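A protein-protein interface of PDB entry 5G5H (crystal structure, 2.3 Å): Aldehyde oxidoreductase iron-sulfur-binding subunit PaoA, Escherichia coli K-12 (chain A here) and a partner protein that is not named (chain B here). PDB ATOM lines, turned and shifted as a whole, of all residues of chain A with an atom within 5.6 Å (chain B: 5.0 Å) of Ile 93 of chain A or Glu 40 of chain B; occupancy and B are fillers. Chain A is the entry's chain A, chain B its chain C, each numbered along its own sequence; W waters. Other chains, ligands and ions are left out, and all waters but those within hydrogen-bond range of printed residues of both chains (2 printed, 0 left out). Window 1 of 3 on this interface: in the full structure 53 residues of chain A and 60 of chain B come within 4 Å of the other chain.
The backbone NH (N) of Tyr 37 of chain B sits at hydrogen-bond distance from the side-chain carboxylate (OE1) of Glu 40 of chain B, 3.1 Å away.
ND1 of His 42 of chain B sits close to NH1 of Arg 36 of chain B, 3.3 Å away.
O of Glu 40 of chain B is in hydrogen-bond range of NH1 of Arg 36 of chain B (2.7 Å).
The side-chain amino group of Lys 96 of chain A lies within hydrogen-bond range of the backbone carbonyl oxygen of Ile 93 of chain A (2.7 Å).
O of Glu 40 of chain B is in hydrogen-bond range of ND1 of His 42 of chain B.
The backbone carbonyl oxygen (O) of Leu 86 of chain A lies within hydrogen-bond range of the backbone NH (N) of His 91 of chain A, 3.0 Å away.
OH of Tyr 37 of chain B sits at hydrogen-bond distance from N of Tyr 160 of chain A, 3.5 Å away.
The side-chain carboxylate (OE2) of Glu 40 of chain B lies within salt-bridge range of the guanidinium group (NH1) of Arg 87 of chain A (3.0 Å).
The side-chain amino group (NZ) of Lys 96 of chain A is in salt-bridge range of the side-chain carboxylate (OE1) of Glu 40 of chain B, at 2.8 Å.
Ile 93 of chain A touches five residues of chain B.
Glu 40 of chain B touches four residues of chain A.
Printed residues of chain B within 4 Å of Lys 96 of chain A: Ala 35, Tyr 37 and Glu 40.
Printed residues of chain B within 4 Å of Arg 87 of chain A: Tyr 39 (3.8 Å) and Glu 40 (3.0 Å).
Of the printed residues of chain B, His 91 of chain A touches His 42.
Thr 34 of chain B touches none of the printed residues of chain A.
The nearest printed residue of chain B that does not touch Gly 94 of chain A is Thr 34 of chain B (5.2 Å).
Arg 87 of chain A touches Tyr 39 of chain B (NH2 to CD2, 3.8 Å).
His 42 of chain B touches His 91 of chain A (CE1 to O, 3.3 Å).
Ile 93 of chain A touches Gly 33 of chain B (CD1 to O, 3.6 Å).
Ile 93 of chain A touches Ala 35 of chain B.
Ile 93 of chain A touches Glu 40 of chain B.
His 42 of chain B touches Ile 93 of chain A.
CA of Gly 94 of chain A touches O of Gly 33 of chain B, at 3.3 Å.
Lys 96 of chain A touches Ala 35 of chain B (NZ to O, 3.6 Å).
NZ of Lys 96 of chain A touches CD1 of Tyr 37 of chain B, at 3.9 Å.
Gly 33 of chain B touches Glu 135 of chain A.
Water W2 lies within hydrogen-bond range of OH of Tyr 160 of chain A (2.5 Å), OE2 of Glu 40 of chain B (2.6 Å) and NH2 of Arg 87 of chain A (2.9 Å).
Water W1 bridges O of Ala 35 of chain B (2.7 Å) and NZ of Lys 96 of chain A (2.9 Å).
Of the 10 printed residues of chain A, 7 touch a printed residue of chain B.
Printed residues of chain A that touch a printed residue of chain B: Arg 87, His 91, Ile 93, Gly 94, Lys 96, Glu 135 and Tyr 160.
Hydrophobic or aromatic side chains of chain A within 4 Å of the printed part of chain B: His 91, Ile 93 and Tyr 160.
Of the 10 printed residues of chain B, 7 touch a printed residue of chain A.
Hydrophobic or aromatic side chains of chain B within 4 Å of the printed part of chain A: Tyr 37, Tyr 39 and His 42.
Along chain B the printed residues that touch a printed residue of chain A span positions 33 to 42.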
ATOM      1  N   LEU A  86      23.638  -9.888  17.984  1.00  0.00           N
ATOM      2  CA  LEU A  86      22.356  -9.194  18.037  1.00  0.00           C
ATOM      3  C   LEU A  86      22.397  -7.871  17.274  1.00  0.00           C
ATOM      4  O   LEU A  86      21.556  -7.610  16.429  1.00  0.00           O
ATOM      5  CB  LEU A  86      21.932  -8.964  19.479  1.00  0.00           C
ATOM      6  CG  LEU A  86      21.691 -10.245  20.283  1.00  0.00           C
ATOM      7  CD1 LEU A  86      21.688  -9.920  21.775  1.00  0.00           C
ATOM      8  CD2 LEU A  86      20.423 -10.963  19.856  1.00  0.00           C
ATOM      9  N   ARG A  87      23.409  -7.065  17.559  1.00  0.00           N
ATOM     10  CA  ARG A  87      23.536  -5.728  16.983  1.00  0.00           C
ATOM     11  C   ARG A  87      23.919  -5.740  15.517  1.00  0.00           C
ATOM     12  O   ARG A  87      23.270  -5.083  14.707  1.00  0.00           O
ATOM     13  CB  ARG A  87      24.551  -4.903  17.780  1.00  0.00           C
ATOM     14  CG  ARG A  87      24.098  -4.546  19.192  1.00  0.00           C
ATOM     15  CD  ARG A  87      25.273  -4.102  20.065  1.00  0.00           C
ATOM     16  NE  ARG A  87      25.979  -2.938  19.514  1.00  0.00           N
ATOM     17  CZ  ARG A  87      25.555  -1.670  19.564  1.00  0.00           C
ATOM     18  NH1 ARG A  87      24.394  -1.349  20.135  1.00  0.00           N
ATOM     19  NH2 ARG A  87      26.293  -0.709  19.015  1.00  0.00           N
ATOM     20  N   HIS A  91      20.788  -7.078  13.573  1.00  0.00           N
ATOM     21  CA  HIS A  91      20.336  -5.671  13.567  1.00  0.00           C
ATOM     22  C   HIS A  91      19.353  -5.327  14.673  1.00  0.00           C
ATOM     23  O   HIS A  91      18.558  -4.410  14.510  1.00  0.00           O
ATOM     24  CB  HIS A  91      19.783  -5.269  12.187  1.00  0.00           C
ATOM     25  CG  HIS A  91      20.609  -5.778  11.060  1.00  0.00           C
ATOM     26  ND1 HIS A  91      21.961  -5.536  10.971  1.00  0.00           N
ATOM     27  CD2 HIS A  91      20.296  -6.576  10.015  1.00  0.00           C
ATOM     28  CE1 HIS A  91      22.446  -6.148   9.904  1.00  0.00           C
ATOM     29  NE2 HIS A  91      21.456  -6.789   9.310  1.00  0.00           N
ATOM     30  N   LEU A  92      19.408  -6.071  15.777  1.00  0.00           N
ATOM     31  CA  LEU A  92      18.668  -5.758  16.997  1.00  0.00           C
ATOM     32  C   LEU A  92      19.581  -4.884  17.863  1.00  0.00           C
ATOM     33  O   LEU A  92      20.312  -5.361  18.716  1.00  0.00           O
ATOM     34  CB  LEU A  92      18.252  -7.031  17.727  1.00  0.00           C
ATOM     35  CG  LEU A  92      17.377  -7.980  16.906  1.00  0.00           C
ATOM     36  CD1 LEU A  92      17.262  -9.314  17.618  1.00  0.00           C
ATOM     37  CD2 LEU A  92      15.996  -7.389  16.653  1.00  0.00           C
ATOM     38  N   ILE A  93      19.523  -3.591  17.591  1.00  0.00           N
ATOM     39  CA  ILE A  93      20.403  -2.598  18.166  1.00  0.00           C
ATOM     40  C   ILE A  93      20.001  -2.109  19.571  1.00  0.00           C
ATOM     41  O   ILE A  93      20.722  -1.305  20.165  1.00  0.00           O
ATOM     42  CB  ILE A  93      20.607  -1.395  17.197  1.00  0.00           C
ATOM     43  CG1 ILE A  93      19.300  -0.620  16.910  1.00  0.00           C
ATOM     44  CG2 ILE A  93      21.251  -1.863  15.908  1.00  0.00           C
ATOM     45  CD1 ILE A  93      19.014   0.534  17.862  1.00  0.00           C
ATOM     46  N   GLY A  94      18.877  -2.588  20.107  1.00  0.00           N
ATOM     47  CA  GLY A  94      18.458  -2.218  21.455  1.00  0.00           C
ATOM     48  C   GLY A  94      19.444  -2.584  22.562  1.00  0.00           C
ATOM     49  O   GLY A  94      19.607  -1.846  23.548  1.00  0.00           O
ATOM     50  N   THR A  95      20.091  -3.737  22.405  1.00  0.00           N
ATOM     51  CA  THR A  95      21.171  -4.141  23.300  1.00  0.00           C
ATOM     52  C   THR A  95      22.410  -3.294  22.971  1.00  0.00           C
ATOM     53  O   THR A  95      22.792  -3.184  21.809  1.00  0.00           O
ATOM     54  CB  THR A  95      21.452  -5.645  23.176  1.00  0.00           C
ATOM     55  OG1 THR A  95      20.243  -6.353  23.442  1.00  0.00           O
ATOM     56  CG2 THR A  95      22.488  -6.102  24.174  1.00  0.00           C
ATOM     57  N   LYS A  96      23.000  -2.684  24.003  1.00  0.00           N
ATOM     58  CA  LYS A  96      24.063  -1.680  23.823  1.00  0.00           C
ATOM     59  C   LYS A  96      25.434  -2.165  24.236  1.00  0.00           C
ATOM     60  O   LYS A  96      25.570  -3.116  25.003  1.00  0.00           O
ATOM     61  CB  LYS A  96      23.718  -0.407  24.599  1.00  0.00           C
ATOM     62  CG  LYS A  96      22.363   0.184  24.260  1.00  0.00           C
ATOM     63  CD  LYS A  96      22.182   0.509  22.786  1.00  0.00           C
ATOM     64  CE  LYS A  96      20.816   1.146  22.546  1.00  0.00           C
ATOM     65  NZ  LYS A  96      20.364   1.170  21.123  1.00  0.00           N
ATOM     66  N   GLU A 135      13.905  -5.438  23.031  1.00  0.00           N
ATOM     67  CA  GLU A 135      12.877  -5.410  21.990  1.00  0.00           C
ATOM     68  C   GLU A 135      11.789  -6.465  22.232  1.00  0.00           C
ATOM     69  O   GLU A 135      10.613  -6.246  21.906  1.00  0.00           O
ATOM     70  CB  GLU A 135      13.502  -5.574  20.594  1.00  0.00           C
ATOM     71  CG  GLU A 135      14.428  -4.421  20.180  1.00  0.00           C
ATOM     72  CD  GLU A 135      15.934  -4.746  20.244  1.00  0.00           C
ATOM     73  OE1 GLU A 135      16.378  -5.571  21.085  1.00  0.00           O
ATOM     74  OE2 GLU A 135      16.693  -4.146  19.440  1.00  0.00           O
ATOM     75  N   TYR A 160      21.337   5.155  27.125  1.00  0.00           N
ATOM     76  CA  TYR A 160      22.287   4.161  26.636  1.00  0.00           C
ATOM     77  C   TYR A 160      22.432   2.961  27.593  1.00  0.00           C
ATOM     78  O   TYR A 160      22.660   1.837  27.130  1.00  0.00           O
ATOM     79  CB  TYR A 160      23.657   4.783  26.327  1.00  0.00           C
ATOM     80  CG  TYR A 160      24.465   3.931  25.373  1.00  0.00           C
ATOM     81  CD1 TYR A 160      24.125   3.882  24.016  1.00  0.00           C
ATOM     82  CD2 TYR A 160      25.558   3.155  25.804  1.00  0.00           C
ATOM     83  CE1 TYR A 160      24.835   3.094  23.119  1.00  0.00           C
ATOM     84  CE2 TYR A 160      26.266   2.361  24.910  1.00  0.00           C
ATOM     85  CZ  TYR A 160      25.906   2.341  23.561  1.00  0.00           C
ATOM     86  OH  TYR A 160      26.566   1.562  22.617  1.00  0.00           O
ATOM     87  N   GLY B  33      14.670   0.192  23.200  1.00  0.00           N
ATOM     88  CA  GLY B  33      15.795  -0.065  22.323  1.00  0.00           C
ATOM     89  C   GLY B  33      15.577   0.346  20.884  1.00  0.00           C
ATOM     90  O   GLY B  33      16.224  -0.216  20.004  1.00  0.00           O
ATOM     91  N   THR B  34      14.690   1.320  20.646  1.00  0.00           N
ATOM     92  CA  THR B  34      14.447   1.841  19.306  1.00  0.00           C
ATOM     93  C   THR B  34      15.044   3.236  19.039  1.00  0.00           C
ATOM     94  O   THR B  34      15.005   3.705  17.916  1.00  0.00           O
ATOM     95  CB  THR B  34      12.950   1.785  18.957  1.00  0.00           C
ATOM     96  OG1 THR B  34      12.186   2.418  19.979  1.00  0.00           O
ATOM     97  CG2 THR B  34      12.485   0.328  18.833  1.00  0.00           C
ATOM     98  N   ALA B  35      15.613   3.904  20.036  1.00  0.00           N
ATOM     99  CA  ALA B  35      16.434   5.108  19.762  1.00  0.00           C
ATOM    100  C   ALA B  35      17.783   4.680  19.143  1.00  0.00           C
ATOM    101  O   ALA B  35      18.426   3.787  19.670  1.00  0.00           O
ATOM    102  CB  ALA B  35      16.672   5.897  21.037  1.00  0.00           C
ATOM    103  N   ARG B  36      18.178   5.299  18.027  1.00  0.00           N
ATOM    104  CA  ARG B  36      19.410   4.935  17.300  1.00  0.00           C
ATOM    105  C   ARG B  36      20.572   5.856  17.668  1.00  0.00           C
ATOM    106  O   ARG B  36      20.504   7.077  17.461  1.00  0.00           O
ATOM    107  CB  ARG B  36      19.233   5.021  15.776  1.00  0.00           C
ATOM    108  CG  ARG B  36      18.126   4.190  15.135  1.00  0.00           C
ATOM    109  CD  ARG B  36      18.260   2.733  15.457  1.00  0.00           C
ATOM    110  NE  ARG B  36      17.279   1.950  14.724  1.00  0.00           N
ATOM    111  CZ  ARG B  36      17.499   1.265  13.598  1.00  0.00           C
ATOM    112  NH1 ARG B  36      18.706   1.219  13.016  1.00  0.00           N
ATOM    113  NH2 ARG B  36      16.486   0.607  13.045  1.00  0.00           N
ATOM    114  N   TYR B  37      21.636   5.253  18.178  1.00  0.00           N
ATOM    115  CA  TYR B  37      22.894   5.943  18.426  1.00  0.00           C
ATOM    116  C   TYR B  37      23.829   5.688  17.239  1.00  0.00           C
ATOM    117  O   TYR B  37      23.519   4.915  16.349  1.00  0.00           O
ATOM    118  CB  TYR B  37      23.497   5.505  19.777  1.00  0.00           C
ATOM    119  CG  TYR B  37      22.581   5.769  20.965  1.00  0.00           C
ATOM    120  CD1 TYR B  37      21.538   4.909  21.255  1.00  0.00           C
ATOM    121  CD2 TYR B  37      22.761   6.865  21.797  1.00  0.00           C
ATOM    122  CE1 TYR B  37      20.693   5.126  22.325  1.00  0.00           C
ATOM    123  CE2 TYR B  37      21.910   7.093  22.869  1.00  0.00           C
ATOM    124  CZ  TYR B  37      20.875   6.214  23.119  1.00  0.00           C
ATOM    125  OH  TYR B  37      20.003   6.400  24.157  1.00  0.00           O
ATOM    126  N   ALA B  38      24.963   6.369  17.236  1.00  0.00           N
ATOM    127  CA  ALA B  38      25.840   6.508  16.057  1.00  0.00           C
ATOM    128  C   ALA B  38      26.232   5.221  15.324  1.00  0.00           C
ATOM    129  O   ALA B  38      26.330   5.237  14.117  1.00  0.00           O
ATOM    130  CB  ALA B  38      27.100   7.267  16.443  1.00  0.00           C
ATOM    131  N   TYR B  39      26.457   4.137  16.059  1.00  0.00           N
ATOM    132  CA  TYR B  39      26.951   2.883  15.509  1.00  0.00           C
ATOM    133  C   TYR B  39      25.835   1.941  15.060  1.00  0.00           C
ATOM    134  O   TYR B  39      26.131   0.793  14.696  1.00  0.00           O
ATOM    135  CB  TYR B  39      27.762   2.169  16.581  1.00  0.00           C
ATOM    136  CG  TYR B  39      28.899   1.259  16.122  1.00  0.00           C
ATOM    137  CD1 TYR B  39      30.096   1.787  15.645  1.00  0.00           C
ATOM    138  CD2 TYR B  39      28.800  -0.127  16.251  1.00  0.00           C
ATOM    139  CE1 TYR B  39      31.154   0.957  15.271  1.00  0.00           C
ATOM    140  CE2 TYR B  39      29.847  -0.966  15.888  1.00  0.00           C
ATOM    141  CZ  TYR B  39      31.024  -0.420  15.409  1.00  0.00           C
ATOM    142  OH  TYR B  39      32.053  -1.243  15.071  1.00  0.00           O
ATOM    143  N   GLU B  40      24.579   2.423  15.083  1.00  0.00           N
ATOM    144  CA  GLU B  40      23.375   1.583  14.990  1.00  0.00           C
ATOM    145  C   GLU B  40      22.432   1.906  13.809  1.00  0.00           C
ATOM    146  O   GLU B  40      21.317   1.381  13.733  1.00  0.00           O
ATOM    147  CB  GLU B  40      22.609   1.711  16.314  1.00  0.00           C
ATOM    148  CG  GLU B  40      23.392   1.228  17.534  1.00  0.00           C
ATOM    149  CD  GLU B  40      22.775   1.683  18.856  1.00  0.00           C
ATOM    150  OE1 GLU B  40      21.658   2.244  18.831  1.00  0.00           O
ATOM    151  OE2 GLU B  40      23.400   1.480  19.927  1.00  0.00           O
ATOM    152  N   TRP B  41      22.894   2.752  12.890  1.00  0.00           N
ATOM    153  CA  TRP B  41      22.128   3.154  11.709  1.00  0.00           C
ATOM    154  C   TRP B  41      22.294   2.139  10.554  1.00  0.00           C
ATOM    155  O   TRP B  41      22.869   2.471   9.524  1.00  0.00           O
ATOM    156  CB  TRP B  41      22.588   4.546  11.247  1.00  0.00           C
ATOM    157  CG  TRP B  41      22.326   5.606  12.224  1.00  0.00           C
ATOM    158  CD1 TRP B  41      23.216   6.172  13.081  1.00  0.00           C
ATOM    159  CD2 TRP B  41      21.069   6.224  12.479  1.00  0.00           C
ATOM    160  NE1 TRP B  41      22.596   7.112  13.858  1.00  0.00           N
ATOM    161  CE2 TRP B  41      21.271   7.165  13.505  1.00  0.00           C
ATOM    162  CE3 TRP B  41      19.784   6.075  11.937  1.00  0.00           C
ATOM    163  CZ2 TRP B  41      20.238   7.975  13.983  1.00  0.00           C
ATOM    164  CZ3 TRP B  41      18.753   6.872  12.421  1.00  0.00           C
ATOM    165  CH2 TRP B  41      18.987   7.813  13.427  1.00  0.00           C
ATOM    166  N   HIS B  42      21.788   0.922  10.723  1.00  0.00           N
ATOM    167  CA  HIS B  42      22.022  -0.124   9.709  1.00  0.00           C
ATOM    168  C   HIS B  42      21.420   0.168   8.343  1.00  0.00           C
ATOM    169  O   HIS B  42      22.127   0.013   7.362  1.00  0.00           O
ATOM    170  CB  HIS B  42      21.689  -1.559  10.169  1.00  0.00           C
ATOM    171  CG  HIS B  42      20.371  -1.711  10.852  1.00  0.00           C
ATOM    172  ND1 HIS B  42      20.213  -1.574  12.217  1.00  0.00           N
ATOM    173  CD2 HIS B  42      19.154  -2.051  10.367  1.00  0.00           C
ATOM    174  CE1 HIS B  42      18.948  -1.792  12.540  1.00  0.00           C
ATOM    175  NE2 HIS B  42      18.282  -2.075  11.435  1.00  0.00           N
HETATM  176  O   HOH W   1      17.863   2.356  21.834  1.00  0.00           O
HETATM  177  O   HOH W   2      25.989   1.952  20.186  1.00  0.00           O
